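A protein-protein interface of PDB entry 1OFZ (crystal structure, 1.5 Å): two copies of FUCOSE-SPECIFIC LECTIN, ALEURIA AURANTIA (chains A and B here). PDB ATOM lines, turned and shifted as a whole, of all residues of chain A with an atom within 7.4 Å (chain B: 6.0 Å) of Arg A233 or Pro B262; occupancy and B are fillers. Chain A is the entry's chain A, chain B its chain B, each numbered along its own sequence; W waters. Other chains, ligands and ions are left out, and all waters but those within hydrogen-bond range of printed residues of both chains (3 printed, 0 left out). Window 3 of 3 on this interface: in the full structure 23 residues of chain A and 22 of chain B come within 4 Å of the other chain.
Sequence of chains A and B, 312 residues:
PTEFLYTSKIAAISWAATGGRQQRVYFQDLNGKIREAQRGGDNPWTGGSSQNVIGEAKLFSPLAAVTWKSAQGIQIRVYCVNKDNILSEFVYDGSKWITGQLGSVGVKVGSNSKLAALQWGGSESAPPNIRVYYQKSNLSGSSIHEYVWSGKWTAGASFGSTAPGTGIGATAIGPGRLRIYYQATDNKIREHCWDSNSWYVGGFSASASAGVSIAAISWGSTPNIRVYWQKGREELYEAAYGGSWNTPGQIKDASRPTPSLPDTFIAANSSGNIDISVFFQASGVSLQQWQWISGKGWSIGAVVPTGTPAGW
OG of Ser A283 lies within hydrogen-bond range of OD2 of Asp B263 (2.8 Å).
The side-chain hydroxyl of Tyr A6 is in hydrogen-bond range of the backbone carbonyl oxygen of Pro A262 (2.6 Å). NH1 of Arg A233 lies within hydrogen-bond range of O of Thr A258, at 3.5 Å. The guanidinium group (NH1) of Arg A233 is in hydrogen-bond range of the backbone carbonyl oxygen (O) of Ser A260 (2.9 Å). The backbone carbonyl oxygen of Leu A261 sits at hydrogen-bond distance from the backbone NH of Arg A233, 3.5 Å away. The side-chain hydroxyl (OG1) of Thr A264 lies within hydrogen-bond range of the backbone carbonyl oxygen (O) of Leu A261. N of Leu A261 sits at hydrogen-bond distance from O of Gln A281, at 3.0 Å.
Among the printed residues, merely in contact across the chains: Tyr A6 with Tyr B6, Tyr A6 with Leu B261, Arg A233 with Pro B262, Leu A261 with Tyr B6, Leu A261 with Pro B262, Pro A262 with Arg B233, Pro A262 with Leu B261 and Pro A262 with Pro B262.
Arg A233 touches just one residue of chain B: Pro B262. Of the printed residues of chain B, Leu A261 touches Tyr B6 (3.7 Å) and Pro B262 (3.9 Å). Of the printed residues of chain B, Pro A262 touches Arg B233 (3.3 Å), Leu B261 (3.9 Å) and Pro B262 (3.8 Å). Of the printed residues of chain A, Leu B261 touches Tyr A6 and Pro A262. The nearest printed residue of chain B that does not touch Arg A233 is Arg B233 (5.4 Å).
Of the 18 printed residues of chain A, 5 touch a printed residue of chain B. Along chain A the printed residues that touch a printed residue of chain B span positions 6 to 283. Of the 9 printed residues of chain B, 5 touch a printed residue of chain A. Hydrophobic or aromatic side chains of chain B that line the printed part of chain A: Tyr B6, Leu B261 and Pro B262. Among the printed residues, 9 pairs touch across the chains. Among the printed residues, no Asp or Glu carboxylate lies within 4 Å of a Lys or Arg side-chain nitrogen of the other chain.
Tyr B6 touches its own counterpart, Tyr A6. Tyr A6 touches Leu B261, and with the chains exchanged Leu A261 touches Tyr B6. Arg A233 touches Pro B262, and with the chains exchanged Pro A262 touches Arg B233. Pro A262 touches its own counterpart, Pro B262. 8 positions are printed for both chains. Of the 9 pairs that touch across the chains among the printed residues, 8 have their exchanged pair printed and touching as well.
Water W1 lies within hydrogen-bond range of OD2 of Asp A263 (2.7 Å) and NH2 of Arg B233 (3.3 Å). Water W2 lies within hydrogen-bond range of the side-chain carboxylate of Asp B263, the side-chain hydroxyl of Tyr B6 and the side-chain hydroxyl of Ser A283. Water W3 lies within hydrogen-bond range of OD2 of Asp B263 (2.7 Å) and NH2 of Arg A233 (3.2 Å).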
ATOM      1  N   TYR A   6      27.789 -16.306 -11.548  1.00  0.00           N
ATOM      2  CA  TYR A   6      27.723 -15.474 -12.741  1.00  0.00           C
ATOM      3  C   TYR A   6      28.103 -14.035 -12.388  1.00  0.00           C
ATOM      4  O   TYR A   6      27.586 -13.440 -11.428  1.00  0.00           O
ATOM      5  CB  TYR A   6      26.335 -15.508 -13.348  1.00  0.00           C
ATOM      6  CG  TYR A   6      26.108 -14.528 -14.469  1.00  0.00           C
ATOM      7  CD1 TYR A   6      26.920 -14.516 -15.598  1.00  0.00           C
ATOM      8  CD2 TYR A   6      25.110 -13.587 -14.395  1.00  0.00           C
ATOM      9  CE1 TYR A   6      26.704 -13.616 -16.625  1.00  0.00           C
ATOM     10  CE2 TYR A   6      24.891 -12.682 -15.419  1.00  0.00           C
ATOM     11  CZ  TYR A   6      25.699 -12.675 -16.516  1.00  0.00           C
ATOM     12  OH  TYR A   6      25.474 -11.789 -17.567  1.00  0.00           O
ATOM     13  N   GLN A 230      38.085  -6.796 -22.618  1.00  0.00           N
ATOM     14  CA  GLN A 230      36.885  -7.420 -23.132  1.00  0.00           C
ATOM     15  C   GLN A 230      35.658  -6.913 -22.434  1.00  0.00           C
ATOM     16  O   GLN A 230      35.624  -6.841 -21.221  1.00  0.00           O
ATOM     17  CB  GLN A 230      36.991  -8.931 -22.926  1.00  0.00           C
ATOM     18  CG  GLN A 230      35.877  -9.736 -23.510  1.00  0.00           C
ATOM     19  CD  GLN A 230      35.957 -11.158 -23.047  1.00  0.00           C
ATOM     20  OE1 GLN A 230      36.629 -11.970 -23.695  1.00  0.00           O
ATOM     21  NE2 GLN A 230      35.311 -11.454 -21.926  1.00  0.00           N
ATOM     22  N   LYS A 231      34.673  -6.532 -23.228  1.00  0.00           N
ATOM     23  CA  LYS A 231      33.340  -6.289 -22.720  1.00  0.00           C
ATOM     24  C   LYS A 231      32.603  -7.593 -22.902  1.00  0.00           C
ATOM     25  O   LYS A 231      32.687  -8.196 -23.974  1.00  0.00           O
ATOM     26  CB  LYS A 231      32.670  -5.188 -23.505  1.00  0.00           C
ATOM     27  CG  LYS A 231      31.233  -4.957 -23.072  1.00  0.00           C
ATOM     28  CD  LYS A 231      30.683  -3.620 -23.504  1.00  0.00           C
ATOM     29  CE  LYS A 231      29.360  -3.374 -22.765  1.00  0.00           C
ATOM     30  NZ  LYS A 231      29.563  -3.037 -21.306  1.00  0.00           N
ATOM     31  N   GLY A 232      31.831  -8.018 -21.906  1.00  0.00           N
ATOM     32  CA  GLY A 232      31.133  -9.297 -22.023  1.00  0.00           C
ATOM     33  C   GLY A 232      30.227  -9.321 -23.250  1.00  0.00           C
ATOM     34  O   GLY A 232      29.538  -8.338 -23.588  1.00  0.00           O
ATOM     35  N   ARG A 233      30.205 -10.460 -23.935  1.00  0.00           N
ATOM     36  CA  ARG A 233      29.470 -10.648 -25.195  1.00  0.00           C
ATOM     37  C   ARG A 233      30.009  -9.824 -26.374  1.00  0.00           C
ATOM     38  O   ARG A 233      29.335  -9.669 -27.399  1.00  0.00           O
ATOM     39  CB  ARG A 233      27.964 -10.454 -25.007  1.00  0.00           C
ATOM     40  CG  ARG A 233      27.196 -11.753 -24.873  1.00  0.00           C
ATOM     41  CD  ARG A 233      27.212 -12.638 -26.103  1.00  0.00           C
ATOM     42  NE  ARG A 233      26.220 -13.706 -26.013  1.00  0.00           N
ATOM     43  CZ  ARG A 233      26.384 -14.880 -25.403  1.00  0.00           C
ATOM     44  NH1 ARG A 233      27.499 -15.200 -24.787  1.00  0.00           N
ATOM     45  NH2 ARG A 233      25.395 -15.776 -25.430  1.00  0.00           N
ATOM     46  N   GLU A 234      31.230  -9.355 -26.237  1.00  0.00           N
ATOM     47  CA  GLU A 234      32.023  -8.843 -27.331  1.00  0.00           C
ATOM     48  C   GLU A 234      33.309  -9.677 -27.376  1.00  0.00           C
ATOM     49  O   GLU A 234      33.572 -10.495 -26.497  1.00  0.00           O
ATOM     50  CB  GLU A 234      32.401  -7.376 -27.128  1.00  0.00           C
ATOM     51  CG  GLU A 234      31.233  -6.409 -27.119  1.00  0.00           C
ATOM     52  CD  GLU A 234      31.700  -4.942 -27.076  1.00  0.00           C
ATOM     53  OE1 GLU A 234      32.926  -4.653 -27.148  1.00  0.00           O
ATOM     54  OE2 GLU A 234      30.793  -4.079 -26.956  1.00  0.00           O
ATOM     55  N   GLU A 235      34.132  -9.466 -28.389  1.00  0.00           N
ATOM     56  CA  GLU A 235      35.390 -10.197 -28.462  1.00  0.00           C
ATOM     57  C   GLU A 235      36.477  -9.572 -27.577  1.00  0.00           C
ATOM     58  O   GLU A 235      36.449  -8.377 -27.237  1.00  0.00           O
ATOM     59  CB  GLU A 235      35.907 -10.321 -29.914  1.00  0.00           C
ATOM     60  CG  GLU A 235      34.911 -10.833 -30.950  1.00  0.00           C
ATOM     61  CD  GLU A 235      34.512 -12.306 -30.819  1.00  0.00           C
ATOM     62  OE1 GLU A 235      34.929 -13.013 -29.882  1.00  0.00           O
ATOM     63  OE2 GLU A 235      33.700 -12.757 -31.665  1.00  0.00           O
ATOM     64  N   PRO A 257      31.578 -17.091 -32.126  1.00  0.00           N
ATOM     65  CA  PRO A 257      31.612 -15.653 -31.871  1.00  0.00           C
ATOM     66  C   PRO A 257      31.249 -15.297 -30.421  1.00  0.00           C
ATOM     67  O   PRO A 257      30.422 -15.955 -29.785  1.00  0.00           O
ATOM     68  CB  PRO A 257      30.540 -15.082 -32.824  1.00  0.00           C
ATOM     69  CG  PRO A 257      30.400 -16.137 -33.867  1.00  0.00           C
ATOM     70  CD  PRO A 257      30.634 -17.443 -33.211  1.00  0.00           C
ATOM     71  N   THR A 258      31.884 -14.236 -29.953  1.00  0.00           N
ATOM     72  CA  THR A 258      31.613 -13.605 -28.649  1.00  0.00           C
ATOM     73  C   THR A 258      31.145 -14.590 -27.586  1.00  0.00           C
ATOM     74  O   THR A 258      29.997 -14.528 -27.107  1.00  0.00           O
ATOM     75  CB  THR A 258      30.581 -12.454 -28.767  1.00  0.00           C
ATOM     76  OG1 THR A 258      29.333 -12.948 -29.258  1.00  0.00           O
ATOM     77  CG2 THR A 258      31.020 -11.349 -29.750  1.00  0.00           C
ATOM     78  N   PRO A 259      32.024 -15.495 -27.181  1.00  0.00           N
ATOM     79  CA  PRO A 259      31.629 -16.579 -26.293  1.00  0.00           C
ATOM     80  C   PRO A 259      31.362 -16.170 -24.841  1.00  0.00           C
ATOM     81  O   PRO A 259      30.704 -16.887 -24.114  1.00  0.00           O
ATOM     82  CB  PRO A 259      32.813 -17.556 -26.408  1.00  0.00           C
ATOM     83  CG  PRO A 259      33.969 -16.710 -26.722  1.00  0.00           C
ATOM     84  CD  PRO A 259      33.426 -15.620 -27.630  1.00  0.00           C
ATOM     85  N   SER A 260      31.875 -15.018 -24.431  1.00  0.00           N
ATOM     86  CA  SER A 260      31.670 -14.580 -23.054  1.00  0.00           C
ATOM     87  C   SER A 260      30.245 -14.086 -22.860  1.00  0.00           C
ATOM     88  O   SER A 260      29.647 -13.551 -23.809  1.00  0.00           O
ATOM     89  CB  SER A 260      32.679 -13.485 -22.697  1.00  0.00           C
ATOM     90  OG  SER A 260      32.388 -12.306 -23.402  1.00  0.00           O
ATOM     91  N   LEU A 261      29.718 -14.210 -21.653  1.00  0.00           N
ATOM     92  CA  LEU A 261      28.391 -13.700 -21.321  1.00  0.00           C
ATOM     93  C   LEU A 261      28.469 -12.187 -21.055  1.00  0.00           C
ATOM     94  O   LEU A 261      29.539 -11.662 -20.747  1.00  0.00           O
ATOM     95  CB  LEU A 261      27.843 -14.380 -20.093  1.00  0.00           C
ATOM     96  CG  LEU A 261      27.487 -15.855 -20.322  1.00  0.00           C
ATOM     97  CD1 LEU A 261      27.230 -16.533 -18.996  1.00  0.00           C
ATOM     98  CD2 LEU A 261      26.227 -16.051 -21.211  1.00  0.00           C
ATOM     99  N   PRO A 262      27.330 -11.501 -21.091  1.00  0.00           N
ATOM    100  CA  PRO A 262      27.341 -10.079 -20.728  1.00  0.00           C
ATOM    101  C   PRO A 262      27.848  -9.822 -19.316  1.00  0.00           C
ATOM    102  O   PRO A 262      27.633 -10.633 -18.399  1.00  0.00           O
ATOM    103  CB  PRO A 262      25.874  -9.668 -20.869  1.00  0.00           C
ATOM    104  CG  PRO A 262      25.310 -10.655 -21.824  1.00  0.00           C
ATOM    105  CD  PRO A 262      25.984 -11.942 -21.501  1.00  0.00           C
ATOM    106  N   ASP A 263      28.490  -8.653 -19.159  1.00  0.00           N
ATOM    107  CA  ASP A 263      28.839  -8.129 -17.839  1.00  0.00           C
ATOM    108  C   ASP A 263      29.808  -9.005 -17.048  1.00  0.00           C
ATOM    109  O   ASP A 263      29.852  -8.949 -15.808  1.00  0.00           O
ATOM    110  CB  ASP A 263      27.572  -7.878 -17.044  1.00  0.00           C
ATOM    111  CG  ASP A 263      26.613  -6.981 -17.784  1.00  0.00           C
ATOM    112  OD1 ASP A 263      27.055  -5.883 -18.220  1.00  0.00           O
ATOM    113  OD2 ASP A 263      25.435  -7.313 -18.012  1.00  0.00           O
ATOM    114  N   THR A 264      30.608  -9.790 -17.769  1.00  0.00           N
ATOM    115  CA  THR A 264      31.574 -10.670 -17.166  1.00  0.00           C
ATOM    116  C   THR A 264      33.007 -10.108 -17.235  1.00  0.00           C
ATOM    117  O   THR A 264      33.225  -8.983 -17.790  1.00  0.00           O
ATOM    118  CB  THR A 264      31.574 -12.053 -17.875  1.00  0.00           C
ATOM    119  OG1 THR A 264      31.796 -11.861 -19.290  1.00  0.00           O
ATOM    120  CG2 THR A 264      30.238 -12.765 -17.661  1.00  0.00           C
ATOM    121  N   GLN A 281      34.196 -15.971 -18.783  1.00  0.00           N
ATOM    122  CA  GLN A 281      33.032 -16.671 -18.295  1.00  0.00           C
ATOM    123  C   GLN A 281      32.009 -16.744 -19.411  1.00  0.00           C
ATOM    124  O   GLN A 281      31.608 -15.738 -19.977  1.00  0.00           O
ATOM    125  CB  GLN A 281      32.435 -15.968 -17.107  1.00  0.00           C
ATOM    126  CG  GLN A 281      31.270 -16.714 -16.451  1.00  0.00           C
ATOM    127  CD  GLN A 281      30.832 -16.083 -15.155  1.00  0.00           C
ATOM    128  OE1 GLN A 281      30.483 -14.903 -15.154  1.00  0.00           O
ATOM    129  NE2 GLN A 281      30.905 -16.823 -14.057  1.00  0.00           N
ATOM    130  N   ALA A 282      31.578 -17.976 -19.691  1.00  0.00           N
ATOM    131  CA  ALA A 282      30.657 -18.280 -20.769  1.00  0.00           C
ATOM    132  C   ALA A 282      29.415 -19.039 -20.263  1.00  0.00           C
ATOM    133  O   ALA A 282      29.288 -19.424 -19.101  1.00  0.00           O
ATOM    134  CB  ALA A 282      31.389 -19.085 -21.779  1.00  0.00           C
ATOM    135  N   SER A 283      28.478 -19.295 -21.185  1.00  0.00           N
ATOM    136  CA  SER A 283      27.297 -20.083 -20.841  1.00  0.00           C
ATOM    137  C   SER A 283      27.741 -21.414 -20.251  1.00  0.00           C
ATOM    138  O   SER A 283      28.772 -21.977 -20.671  1.00  0.00           O
ATOM    139  CB  SER A 283      26.456 -20.329 -22.102  1.00  0.00           C
ATOM    140  OG  SER A 283      25.460 -21.300 -21.840  1.00  0.00           O
ATOM    141  N   TYR B   6      21.353 -16.483 -11.400  1.00  0.00           N
ATOM    142  CA  TYR B   6      21.361 -16.460 -12.866  1.00  0.00           C
ATOM    143  C   TYR B   6      20.959 -17.807 -13.448  1.00  0.00           C
ATOM    144  O   TYR B   6      21.511 -18.832 -13.096  1.00  0.00           O
ATOM    145  CB  TYR B   6      22.736 -16.072 -13.386  1.00  0.00           C
ATOM    146  CG  TYR B   6      22.886 -16.086 -14.869  1.00  0.00           C
ATOM    147  CD1 TYR B   6      22.056 -15.335 -15.702  1.00  0.00           C
ATOM    148  CD2 TYR B   6      23.856 -16.861 -15.485  1.00  0.00           C
ATOM    149  CE1 TYR B   6      22.189 -15.384 -17.078  1.00  0.00           C
ATOM    150  CE2 TYR B   6      23.985 -16.890 -16.851  1.00  0.00           C
ATOM    151  CZ  TYR B   6      23.155 -16.155 -17.652  1.00  0.00           C
ATOM    152  OH  TYR B   6      23.322 -16.190 -18.990  1.00  0.00           O
ATOM    153  N   THR B   7      19.990 -17.748 -14.378  1.00  0.00           N
ATOM    154  CA  THR B   7      19.300 -18.918 -14.949  1.00  0.00           C
ATOM    155  C   THR B   7      18.363 -19.642 -13.989  1.00  0.00           C
ATOM    156  O   THR B   7      17.945 -20.759 -14.238  1.00  0.00           O
ATOM    157  CB  THR B   7      20.194 -19.901 -15.742  1.00  0.00           C
ATOM    158  OG1 THR B   7      20.998 -20.720 -14.862  1.00  0.00           O
ATOM    159  CG2 THR B   7      21.149 -19.151 -16.693  1.00  0.00           C
ATOM    160  N   GLY B 232      16.729 -16.519 -24.447  1.00  0.00           N
ATOM    161  CA  GLY B 232      17.448 -15.451 -23.792  1.00  0.00           C
ATOM    162  C   GLY B 232      18.285 -14.659 -24.789  1.00  0.00           C
ATOM    163  O   GLY B 232      18.934 -15.250 -25.652  1.00  0.00           O
ATOM    164  N   ARG B 233      18.250 -13.336 -24.650  1.00  0.00           N
ATOM    165  CA  ARG B 233      18.908 -12.370 -25.528  1.00  0.00           C
ATOM    166  C   ARG B 233      18.308 -12.302 -26.932  1.00  0.00           C
ATOM    167  O   ARG B 233      18.882 -11.687 -27.861  1.00  0.00           O
ATOM    168  CB  ARG B 233      20.432 -12.625 -25.550  1.00  0.00           C
ATOM    169  CG  ARG B 233      21.339 -11.422 -25.759  1.00  0.00           C
ATOM    170  CD  ARG B 233      21.003 -10.191 -25.022  1.00  0.00           C
ATOM    171  NE  ARG B 233      22.151  -9.480 -24.447  1.00  0.00           N
ATOM    172  CZ  ARG B 233      22.172  -8.975 -23.217  1.00  0.00           C
ATOM    173  NH1 ARG B 233      21.145  -9.101 -22.403  1.00  0.00           N
ATOM    174  NH2 ARG B 233      23.228  -8.298 -22.792  1.00  0.00           N
ATOM    175  N   SER B 260      16.674  -9.535 -22.165  1.00  0.00           N
ATOM    176  CA  SER B 260      16.934 -10.712 -21.350  1.00  0.00           C
ATOM    177  C   SER B 260      18.358 -11.178 -21.536  1.00  0.00           C
ATOM    178  O   SER B 260      18.948 -10.993 -22.595  1.00  0.00           O
ATOM    179  CB  SER B 260      15.987 -11.868 -21.668  1.00  0.00           C
ATOM    180  OG  SER B 260      16.133 -12.318 -22.968  1.00  0.00           O
ATOM    181  N   LEU B 261      18.886 -11.861 -20.528  1.00  0.00           N
ATOM    182  CA  LEU B 261      20.225 -12.444 -20.655  1.00  0.00           C
ATOM    183  C   LEU B 261      20.149 -13.811 -21.338  1.00  0.00           C
ATOM    184  O   LEU B 261      19.101 -14.443 -21.353  1.00  0.00           O
ATOM    185  CB  LEU B 261      20.823 -12.639 -19.273  1.00  0.00           C
ATOM    186  CG  LEU B 261      21.228 -11.344 -18.566  1.00  0.00           C
ATOM    187  CD1 LEU B 261      21.558 -11.648 -17.127  1.00  0.00           C
ATOM    188  CD2 LEU B 261      22.390 -10.695 -19.226  1.00  0.00           C
ATOM    189  N   PRO B 262      21.264 -14.308 -21.875  1.00  0.00           N
ATOM    190  CA  PRO B 262      21.266 -15.640 -22.495  1.00  0.00           C
ATOM    191  C   PRO B 262      20.859 -16.745 -21.508  1.00  0.00           C
ATOM    192  O   PRO B 262      21.134 -16.671 -20.300  1.00  0.00           O
ATOM    193  CB  PRO B 262      22.722 -15.823 -22.963  1.00  0.00           C
ATOM    194  CG  PRO B 262      23.226 -14.410 -23.081  1.00  0.00           C
ATOM    195  CD  PRO B 262      22.592 -13.659 -21.952  1.00  0.00           C
ATOM    196  N   ASP B 263      20.188 -17.771 -22.029  1.00  0.00           N
ATOM    197  CA  ASP B 263      19.899 -18.992 -21.289  1.00  0.00           C
ATOM    198  C   ASP B 263      18.981 -18.829 -20.072  1.00  0.00           C
ATOM    199  O   ASP B 263      18.954 -19.658 -19.169  1.00  0.00           O
ATOM    200  CB  ASP B 263      21.195 -19.715 -20.916  1.00  0.00           C
ATOM    201  CG  ASP B 263      22.088 -19.913 -22.102  1.00  0.00           C
ATOM    202  OD1 ASP B 263      21.602 -20.522 -23.095  1.00  0.00           O
ATOM    203  OD2 ASP B 263      23.270 -19.512 -22.125  1.00  0.00           O
ATOM    204  N   THR B 264      18.136 -17.797 -20.133  1.00  0.00           N
ATOM    205  CA  THR B 264      17.232 -17.477 -19.052  1.00  0.00           C
ATOM    206  C   THR B 264      15.804 -17.937 -19.367  1.00  0.00           C
ATOM    207  O   THR B 264      15.506 -18.437 -20.463  1.00  0.00           O
ATOM    208  CB  THR B 264      17.231 -15.945 -18.779  1.00  0.00           C
ATOM    209  OG1 THR B 264      16.914 -15.211 -19.975  1.00  0.00           O
ATOM    210  CG2 THR B 264      18.608 -15.462 -18.234  1.00  0.00           C
HETATM  211  O   HOH W   1      24.194  -6.407 -20.241  1.00  0.00           O
HETATM  212  O   HOH W   2      24.445 -18.723 -19.804  1.00  0.00           O
HETATM  213  O   HOH W   3      24.367 -18.640 -24.489  1.00  0.00           O
